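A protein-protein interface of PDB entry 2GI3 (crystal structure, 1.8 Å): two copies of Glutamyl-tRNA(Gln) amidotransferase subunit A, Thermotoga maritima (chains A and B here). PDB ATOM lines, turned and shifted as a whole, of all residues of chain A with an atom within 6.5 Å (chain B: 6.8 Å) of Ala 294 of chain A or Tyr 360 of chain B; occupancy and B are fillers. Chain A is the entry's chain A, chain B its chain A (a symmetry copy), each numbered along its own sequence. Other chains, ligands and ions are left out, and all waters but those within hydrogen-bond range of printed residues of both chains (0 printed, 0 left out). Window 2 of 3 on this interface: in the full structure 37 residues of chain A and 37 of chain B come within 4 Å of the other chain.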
ATOM      1  N   LYS A 290      36.934 -38.792  21.808  1.00  0.00           N
ATOM      2  CA  LYS A 290      35.666 -38.338  21.285  1.00  0.00           C
ATOM      3  C   LYS A 290      35.222 -37.027  21.915  1.00  0.00           C
ATOM      4  O   LYS A 290      34.355 -36.376  21.374  1.00  0.00           O
ATOM      5  CB  LYS A 290      34.585 -39.412  21.459  1.00  0.00           C
ATOM      6  CG  LYS A 290      34.157 -39.690  22.896  1.00  0.00           C
ATOM      7  CD  LYS A 290      33.330 -40.999  22.975  1.00  0.00           C
ATOM      8  CE  LYS A 290      33.272 -41.523  24.407  1.00  0.00           C
ATOM      9  NZ  LYS A 290      32.052 -42.377  24.694  1.00  0.00           N
ATOM     10  N   TYR A 291      35.808 -36.640  23.044  1.00  0.00           N
ATOM     11  CA  TYR A 291      35.524 -35.319  23.645  1.00  0.00           C
ATOM     12  C   TYR A 291      36.395 -34.145  23.163  1.00  0.00           C
ATOM     13  O   TYR A 291      36.267 -33.027  23.688  1.00  0.00           O
ATOM     14  CB  TYR A 291      35.613 -35.417  25.170  1.00  0.00           C
ATOM     15  CG  TYR A 291      34.696 -36.509  25.692  1.00  0.00           C
ATOM     16  CD1 TYR A 291      33.322 -36.352  25.661  1.00  0.00           C
ATOM     17  CD2 TYR A 291      35.208 -37.719  26.146  1.00  0.00           C
ATOM     18  CE1 TYR A 291      32.471 -37.368  26.107  1.00  0.00           C
ATOM     19  CE2 TYR A 291      34.380 -38.737  26.584  1.00  0.00           C
ATOM     20  CZ  TYR A 291      33.015 -38.553  26.580  1.00  0.00           C
ATOM     21  OH  TYR A 291      32.192 -39.561  27.036  1.00  0.00           O
ATOM     22  N   SER A 292      37.246 -34.382  22.168  1.00  0.00           N
ATOM     23  CA  SER A 292      38.207 -33.361  21.699  1.00  0.00           C
ATOM     24  C   SER A 292      37.547 -32.082  21.159  1.00  0.00           C
ATOM     25  O   SER A 292      37.882 -30.947  21.569  1.00  0.00           O
ATOM     26  CB  SER A 292      39.140 -33.967  20.623  1.00  0.00           C
ATOM     27  OG  SER A 292      40.005 -34.934  21.205  1.00  0.00           O
ATOM     28  N   VAL A 293      36.593 -32.279  20.266  1.00  0.00           N
ATOM     29  CA  VAL A 293      35.937 -31.166  19.562  1.00  0.00           C
ATOM     30  C   VAL A 293      35.163 -30.322  20.576  1.00  0.00           C
ATOM     31  O   VAL A 293      35.397 -29.130  20.661  1.00  0.00           O
ATOM     32  CB  VAL A 293      35.056 -31.660  18.375  1.00  0.00           C
ATOM     33  CG1 VAL A 293      34.252 -30.507  17.790  1.00  0.00           C
ATOM     34  CG2 VAL A 293      35.931 -32.283  17.260  1.00  0.00           C
ATOM     35  N   ALA A 294      34.305 -30.946  21.389  1.00  0.00           N
ATOM     36  CA  ALA A 294      33.564 -30.221  22.437  1.00  0.00           C
ATOM     37  C   ALA A 294      34.517 -29.483  23.368  1.00  0.00           C
ATOM     38  O   ALA A 294      34.290 -28.328  23.729  1.00  0.00           O
ATOM     39  CB  ALA A 294      32.703 -31.180  23.244  1.00  0.00           C
ATOM     40  N   THR A 295      35.605 -30.137  23.737  1.00  0.00           N
ATOM     41  CA  THR A 295      36.596 -29.508  24.648  1.00  0.00           C
ATOM     42  C   THR A 295      37.242 -28.268  24.002  1.00  0.00           C
ATOM     43  O   THR A 295      37.367 -27.185  24.607  1.00  0.00           O
ATOM     44  CB  THR A 295      37.664 -30.525  25.044  1.00  0.00           C
ATOM     45  OG1 THR A 295      37.042 -31.601  25.783  1.00  0.00           O
ATOM     46  CG2 THR A 295      38.772 -29.862  25.871  1.00  0.00           C
ATOM     47  N   TYR A 296      37.648 -28.433  22.755  1.00  0.00           N
ATOM     48  CA  TYR A 296      38.205 -27.334  21.964  1.00  0.00           C
ATOM     49  C   TYR A 296      37.289 -26.139  21.885  1.00  0.00           C
ATOM     50  O   TYR A 296      37.696 -25.015  22.072  1.00  0.00           O
ATOM     51  CB  TYR A 296      38.498 -27.826  20.548  1.00  0.00           C
ATOM     52  CG  TYR A 296      39.093 -26.759  19.657  1.00  0.00           C
ATOM     53  CD1 TYR A 296      40.463 -26.444  19.708  1.00  0.00           C
ATOM     54  CD2 TYR A 296      38.293 -26.076  18.737  1.00  0.00           C
ATOM     55  CE1 TYR A 296      41.010 -25.450  18.877  1.00  0.00           C
ATOM     56  CE2 TYR A 296      38.837 -25.084  17.898  1.00  0.00           C
ATOM     57  CZ  TYR A 296      40.187 -24.782  17.974  1.00  0.00           C
ATOM     58  OH  TYR A 296      40.679 -23.789  17.167  1.00  0.00           O
ATOM     59  N   TYR A 297      36.030 -26.403  21.582  1.00  0.00           N
ATOM     60  CA  TYR A 297      35.065 -25.310  21.494  1.00  0.00           C
ATOM     61  C   TYR A 297      34.639 -24.644  22.817  1.00  0.00           C
ATOM     62  O   TYR A 297      33.933 -23.634  22.766  1.00  0.00           O
ATOM     63  CB  TYR A 297      33.875 -25.762  20.657  1.00  0.00           C
ATOM     64  CG  TYR A 297      34.252 -25.864  19.208  1.00  0.00           C
ATOM     65  CD1 TYR A 297      34.743 -24.755  18.518  1.00  0.00           C
ATOM     66  CD2 TYR A 297      34.163 -27.070  18.533  1.00  0.00           C
ATOM     67  CE1 TYR A 297      35.116 -24.861  17.167  1.00  0.00           C
ATOM     68  CE2 TYR A 297      34.503 -27.170  17.207  1.00  0.00           C
ATOM     69  CZ  TYR A 297      34.978 -26.071  16.533  1.00  0.00           C
ATOM     70  OH  TYR A 297      35.332 -26.233  15.210  1.00  0.00           O
ATOM     71  N   VAL A 298      35.070 -25.150  23.977  1.00  0.00           N
ATOM     72  CA  VAL A 298      34.984 -24.392  25.234  1.00  0.00           C
ATOM     73  C   VAL A 298      36.248 -23.523  25.386  1.00  0.00           C
ATOM     74  O   VAL A 298      36.205 -22.332  25.775  1.00  0.00           O
ATOM     75  CB  VAL A 298      34.816 -25.352  26.514  1.00  0.00           C
ATOM     76  CG1 VAL A 298      34.846 -24.557  27.828  1.00  0.00           C
ATOM     77  CG2 VAL A 298      33.549 -26.210  26.458  1.00  0.00           C
ATOM     78  N   ILE A 299      37.399 -24.101  25.085  1.00  0.00           N
ATOM     79  CA  ILE A 299      38.648 -23.432  25.419  1.00  0.00           C
ATOM     80  C   ILE A 299      39.003 -22.309  24.440  1.00  0.00           C
ATOM     81  O   ILE A 299      39.343 -21.202  24.847  1.00  0.00           O
ATOM     82  CB  ILE A 299      39.783 -24.473  25.562  1.00  0.00           C
ATOM     83  CG1 ILE A 299      39.458 -25.394  26.752  1.00  0.00           C
ATOM     84  CG2 ILE A 299      41.142 -23.771  25.768  1.00  0.00           C
ATOM     85  CD1 ILE A 299      40.440 -26.537  26.936  1.00  0.00           C
ATOM     86  N   TYR A 356      28.414 -20.281  30.523  1.00  0.00           N
ATOM     87  CA  TYR A 356      28.897 -21.616  30.189  1.00  0.00           C
ATOM     88  C   TYR A 356      30.403 -21.717  30.363  1.00  0.00           C
ATOM     89  O   TYR A 356      30.887 -22.641  31.037  1.00  0.00           O
ATOM     90  CB  TYR A 356      28.487 -21.985  28.768  1.00  0.00           C
ATOM     91  CG  TYR A 356      28.688 -23.443  28.454  1.00  0.00           C
ATOM     92  CD1 TYR A 356      29.934 -23.922  28.027  1.00  0.00           C
ATOM     93  CD2 TYR A 356      27.663 -24.358  28.617  1.00  0.00           C
ATOM     94  CE1 TYR A 356      30.137 -25.282  27.747  1.00  0.00           C
ATOM     95  CE2 TYR A 356      27.855 -25.713  28.342  1.00  0.00           C
ATOM     96  CZ  TYR A 356      29.098 -26.170  27.914  1.00  0.00           C
ATOM     97  OH  TYR A 356      29.295 -27.510  27.634  1.00  0.00           O
ATOM     98  N   ALA A 364      36.710 -28.392  31.148  1.00  0.00           N
ATOM     99  CA  ALA A 364      37.251 -28.583  29.789  1.00  0.00           C
ATOM    100  C   ALA A 364      38.772 -28.736  29.852  1.00  0.00           C
ATOM    101  O   ALA A 364      39.333 -29.558  29.139  1.00  0.00           O
ATOM    102  CB  ALA A 364      36.888 -27.422  28.884  1.00  0.00           C
ATOM    103  N   LEU A 404      26.821 -27.232  12.633  1.00  0.00           N
ATOM    104  CA  LEU A 404      27.478 -28.427  13.135  1.00  0.00           C
ATOM    105  C   LEU A 404      28.460 -29.024  12.102  1.00  0.00           C
ATOM    106  O   LEU A 404      29.599 -29.354  12.445  1.00  0.00           O
ATOM    107  CB  LEU A 404      26.421 -29.451  13.557  1.00  0.00           C
ATOM    108  CG  LEU A 404      26.917 -30.745  14.167  1.00  0.00           C
ATOM    109  CD1 LEU A 404      27.797 -30.431  15.341  1.00  0.00           C
ATOM    110  CD2 LEU A 404      25.698 -31.612  14.532  1.00  0.00           C
ATOM    111  N   VAL B 298      19.966 -25.689  27.356  1.00  0.00           N
ATOM    112  CA  VAL B 298      20.015 -26.188  25.974  1.00  0.00           C
ATOM    113  C   VAL B 298      18.610 -26.079  25.348  1.00  0.00           C
ATOM    114  O   VAL B 298      18.422 -25.663  24.181  1.00  0.00           O
ATOM    115  CB  VAL B 298      20.540 -27.707  25.893  1.00  0.00           C
ATOM    116  CG1 VAL B 298      20.475 -28.255  24.459  1.00  0.00           C
ATOM    117  CG2 VAL B 298      21.956 -27.883  26.449  1.00  0.00           C
ATOM    118  N   ILE B 299      17.597 -26.455  26.111  1.00  0.00           N
ATOM    119  CA  ILE B 299      16.272 -26.602  25.524  1.00  0.00           C
ATOM    120  C   ILE B 299      15.563 -25.261  25.311  1.00  0.00           C
ATOM    121  O   ILE B 299      15.026 -24.995  24.239  1.00  0.00           O
ATOM    122  CB  ILE B 299      15.430 -27.591  26.363  1.00  0.00           C
ATOM    123  CG1 ILE B 299      16.087 -28.981  26.291  1.00  0.00           C
ATOM    124  CG2 ILE B 299      13.977 -27.644  25.843  1.00  0.00           C
ATOM    125  CD1 ILE B 299      15.420 -30.027  27.166  1.00  0.00           C
ATOM    126  N   ALA B 355      25.373 -24.752  16.461  1.00  0.00           N
ATOM    127  CA  ALA B 355      26.036 -26.051  16.342  1.00  0.00           C
ATOM    128  C   ALA B 355      25.809 -26.923  17.605  1.00  0.00           C
ATOM    129  O   ALA B 355      25.517 -28.124  17.511  1.00  0.00           O
ATOM    130  CB  ALA B 355      27.570 -25.852  16.082  1.00  0.00           C
ATOM    131  N   TYR B 356      26.012 -26.318  18.758  1.00  0.00           N
ATOM    132  CA  TYR B 356      25.814 -26.965  20.051  1.00  0.00           C
ATOM    133  C   TYR B 356      24.401 -27.505  20.187  1.00  0.00           C
ATOM    134  O   TYR B 356      24.219 -28.684  20.531  1.00  0.00           O
ATOM    135  CB  TYR B 356      26.138 -25.994  21.181  1.00  0.00           C
ATOM    136  CG  TYR B 356      26.243 -26.664  22.524  1.00  0.00           C
ATOM    137  CD1 TYR B 356      25.100 -26.905  23.299  1.00  0.00           C
ATOM    138  CD2 TYR B 356      27.462 -27.098  23.014  1.00  0.00           C
ATOM    139  CE1 TYR B 356      25.185 -27.543  24.546  1.00  0.00           C
ATOM    140  CE2 TYR B 356      27.557 -27.735  24.252  1.00  0.00           C
ATOM    141  CZ  TYR B 356      26.412 -27.960  25.011  1.00  0.00           C
ATOM    142  OH  TYR B 356      26.498 -28.586  26.242  1.00  0.00           O
ATOM    143  N   TYR B 357      23.402 -26.680  19.861  1.00  0.00           N
ATOM    144  CA  TYR B 357      21.996 -27.128  19.919  1.00  0.00           C
ATOM    145  C   TYR B 357      21.796 -28.301  18.989  1.00  0.00           C
ATOM    146  O   TYR B 357      21.186 -29.302  19.360  1.00  0.00           O
ATOM    147  CB  TYR B 357      20.992 -26.022  19.579  1.00  0.00           C
ATOM    148  CG  TYR B 357      21.106 -24.754  20.410  1.00  0.00           C
ATOM    149  CD1 TYR B 357      21.549 -24.785  21.728  1.00  0.00           C
ATOM    150  CD2 TYR B 357      20.758 -23.505  19.866  1.00  0.00           C
ATOM    151  CE1 TYR B 357      21.657 -23.614  22.487  1.00  0.00           C
ATOM    152  CE2 TYR B 357      20.868 -22.330  20.609  1.00  0.00           C
ATOM    153  CZ  TYR B 357      21.318 -22.395  21.927  1.00  0.00           C
ATOM    154  OH  TYR B 357      21.441 -21.256  22.703  1.00  0.00           O
ATOM    155  N   GLU B 358      22.344 -28.200  17.780  1.00  0.00           N
ATOM    156  CA  GLU B 358      22.263 -29.307  16.854  1.00  0.00           C
ATOM    157  C   GLU B 358      22.896 -30.580  17.416  1.00  0.00           C
ATOM    158  O   GLU B 358      22.353 -31.665  17.253  1.00  0.00           O
ATOM    159  CB  GLU B 358      22.941 -28.992  15.526  1.00  0.00           C
ATOM    160  CG  GLU B 358      22.297 -27.930  14.710  1.00  0.00           C
ATOM    161  CD  GLU B 358      23.004 -27.770  13.379  1.00  0.00           C
ATOM    162  OE1 GLU B 358      24.032 -27.057  13.338  1.00  0.00           O
ATOM    163  OE2 GLU B 358      22.519 -28.379  12.401  1.00  0.00           O
ATOM    164  N   ALA B 359      24.035 -30.460  18.070  1.00  0.00           N
ATOM    165  CA  ALA B 359      24.753 -31.644  18.560  1.00  0.00           C
ATOM    166  C   ALA B 359      24.089 -32.229  19.800  1.00  0.00           C
ATOM    167  O   ALA B 359      24.159 -33.427  20.025  1.00  0.00           O
ATOM    168  CB  ALA B 359      26.183 -31.321  18.870  1.00  0.00           C
ATOM    169  N   TYR B 360      23.442 -31.379  20.588  1.00  0.00           N
ATOM    170  CA  TYR B 360      23.094 -31.736  21.951  1.00  0.00           C
ATOM    171  C   TYR B 360      21.639 -31.658  22.361  1.00  0.00           C
ATOM    172  O   TYR B 360      21.329 -32.079  23.479  1.00  0.00           O
ATOM    173  CB  TYR B 360      23.945 -30.931  22.922  1.00  0.00           C
ATOM    174  CG  TYR B 360      25.401 -31.286  22.797  1.00  0.00           C
ATOM    175  CD1 TYR B 360      25.817 -32.596  22.966  1.00  0.00           C
ATOM    176  CD2 TYR B 360      26.359 -30.332  22.492  1.00  0.00           C
ATOM    177  CE1 TYR B 360      27.132 -32.951  22.836  1.00  0.00           C
ATOM    178  CE2 TYR B 360      27.703 -30.684  22.362  1.00  0.00           C
ATOM    179  CZ  TYR B 360      28.076 -32.003  22.539  1.00  0.00           C
ATOM    180  OH  TYR B 360      29.386 -32.422  22.430  1.00  0.00           O
ATOM    181  N   PHE B 361      20.753 -31.182  21.491  1.00  0.00           N
ATOM    182  CA  PHE B 361      19.338 -31.055  21.850  1.00  0.00           C
ATOM    183  C   PHE B 361      18.731 -32.392  22.227  1.00  0.00           C
ATOM    184  O   PHE B 361      18.060 -32.517  23.237  1.00  0.00           O
ATOM    185  CB  PHE B 361      18.523 -30.447  20.713  1.00  0.00           C
ATOM    186  CG  PHE B 361      17.070 -30.182  21.080  1.00  0.00           C
ATOM    187  CD1 PHE B 361      16.722 -29.079  21.852  1.00  0.00           C
ATOM    188  CD2 PHE B 361      16.062 -31.043  20.658  1.00  0.00           C
ATOM    189  CE1 PHE B 361      15.397 -28.832  22.194  1.00  0.00           C
ATOM    190  CE2 PHE B 361      14.734 -30.793  20.991  1.00  0.00           C
ATOM    191  CZ  PHE B 361      14.404 -29.698  21.768  1.00  0.00           C
ATOM    192  N   ASN B 362      18.938 -33.392  21.383  1.00  0.00           N
ATOM    193  CA  ASN B 362      18.398 -34.716  21.649  1.00  0.00           C
ATOM    194  C   ASN B 362      18.903 -35.284  22.964  1.00  0.00           C
ATOM    195  O   ASN B 362      18.123 -35.851  23.724  1.00  0.00           O
ATOM    196  CB  ASN B 362      18.701 -35.674  20.486  1.00  0.00           C
ATOM    197  CG  ASN B 362      17.776 -35.459  19.292  1.00  0.00           C
ATOM    198  OD1 ASN B 362      16.743 -34.777  19.384  1.00  0.00           O
ATOM    199  ND2 ASN B 362      18.144 -36.042  18.158  1.00  0.00           N
ATOM    200  N   LYS B 363      20.193 -35.146  23.238  1.00  0.00           N
ATOM    201  CA  LYS B 363      20.728 -35.580  24.515  1.00  0.00           C
ATOM    202  C   LYS B 363      20.103 -34.830  25.696  1.00  0.00           C
ATOM    203  O   LYS B 363      19.841 -35.430  26.747  1.00  0.00           O
ATOM    204  CB  LYS B 363      22.232 -35.406  24.569  1.00  0.00           C
ATOM    205  CG  LYS B 363      22.901 -36.076  25.790  1.00  0.00           C
ATOM    206  CD  LYS B 363      23.913 -35.155  26.469  1.00  0.00           C
ATOM    207  N   ALA B 364      19.920 -33.521  25.542  1.00  0.00           N
ATOM    208  CA  ALA B 364      19.290 -32.710  26.602  1.00  0.00           C
ATOM    209  C   ALA B 364      17.861 -33.198  26.849  1.00  0.00           C
ATOM    210  O   ALA B 364      17.428 -33.266  27.991  1.00  0.00           O
ATOM    211  CB  ALA B 364      19.274 -31.239  26.233  1.00  0.00           C
ATOM    212  N   MET B 365      17.146 -33.548  25.784  1.00  0.00           N
ATOM    213  CA  MET B 365      15.816 -34.114  25.921  1.00  0.00           C
ATOM    214  C   MET B 365      15.797 -35.472  26.628  1.00  0.00           C
ATOM    215  O   MET B 365      14.858 -35.760  27.381  1.00  0.00           O
ATOM    216  CB  MET B 365      15.108 -34.205  24.566  1.00  0.00           C
ATOM    217  CG  MET B 365      14.682 -32.825  24.019  1.00  0.00           C
ATOM    218  SD  MET B 365      13.261 -31.838  25.004  1.00  0.00           S
ATOM    219  CE  MET B 365      11.735 -32.967  24.541  1.00  0.00           C
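N of Leu 404 of chain A is in hydrogen-bond range of OE1 of Glu 358 of chain B, 2.9 Å away. OH of Tyr 356 of chain A sits at hydrogen-bond distance from OH of Tyr 356 of chain B (3.3 Å).
Tyr 360 of chain B touches Ala 294 of chain A (OH to CB, 3.6 Å). Leu 404 of chain A touches Ala 355 of chain B (N to CB, 3.8 Å). Leu 404 of chain A touches Ala 359 of chain B (CD1 to CB, 3.98 Å).
Printed residues of chain B within 4 Å of Ala 294 of chain A: Tyr 360 (3.6 Å). Tyr 297 of chain A touches none of the printed residues of chain B. Printed residues of chain B within 4 Å of Tyr 356 of chain A: Tyr 356 (3.3 Å). Ala 364 of chain A touches none of the printed residues of chain B. Of the printed residues of chain B, Leu 404 of chain A touches Ala 355 (3.8 Å), Glu 358 (2.9 Å) and Ala 359 (3.98 Å). Of the printed residues of chain A, Ala 355 of chain B touches Leu 404. Printed residues of chain A within 4 Å of Tyr 356 of chain B: Tyr 356 (3.3 Å). Printed residues of chain A within 4 Å of Ala 359 of chain B: Leu 404. Of chain A, only Ala 294 (3.6 Å) comes within 4 Å of Tyr 360 of chain B. The nearest residue of chain B that does not touch Ala 294 of chain A is Tyr 356 of chain B (6.3 Å). The nearest printed residue of chain A that does not touch Tyr 356 of chain B is Leu 404 of chain A (5.6 Å).
Of the 13 printed residues of chain A, 3 touch a printed residue of chain B. Printed residues of chain A that touch a printed residue of chain B: Ala 294, Tyr 356 and Leu 404. Hydrophobic or aromatic side chains of chain A that line the printed part of chain B: Ala 294, Tyr 356 and Leu 404. Printed residues of chain B that touch a printed residue of chain A: Ala 355, Tyr 356, Glu 358, Ala 359 and Tyr 360. Among the printed residues, no Asp or Glu carboxylate lies within 4 Å of a Lys or Arg side-chain nitrogen of the other chain.
Tyr 356 of chain A touches its own counterpart, Tyr 356 of chain B. Of the 5 pairs that touch across the chains among the printed residues, 1 has its exchanged pair printed and touching as well.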
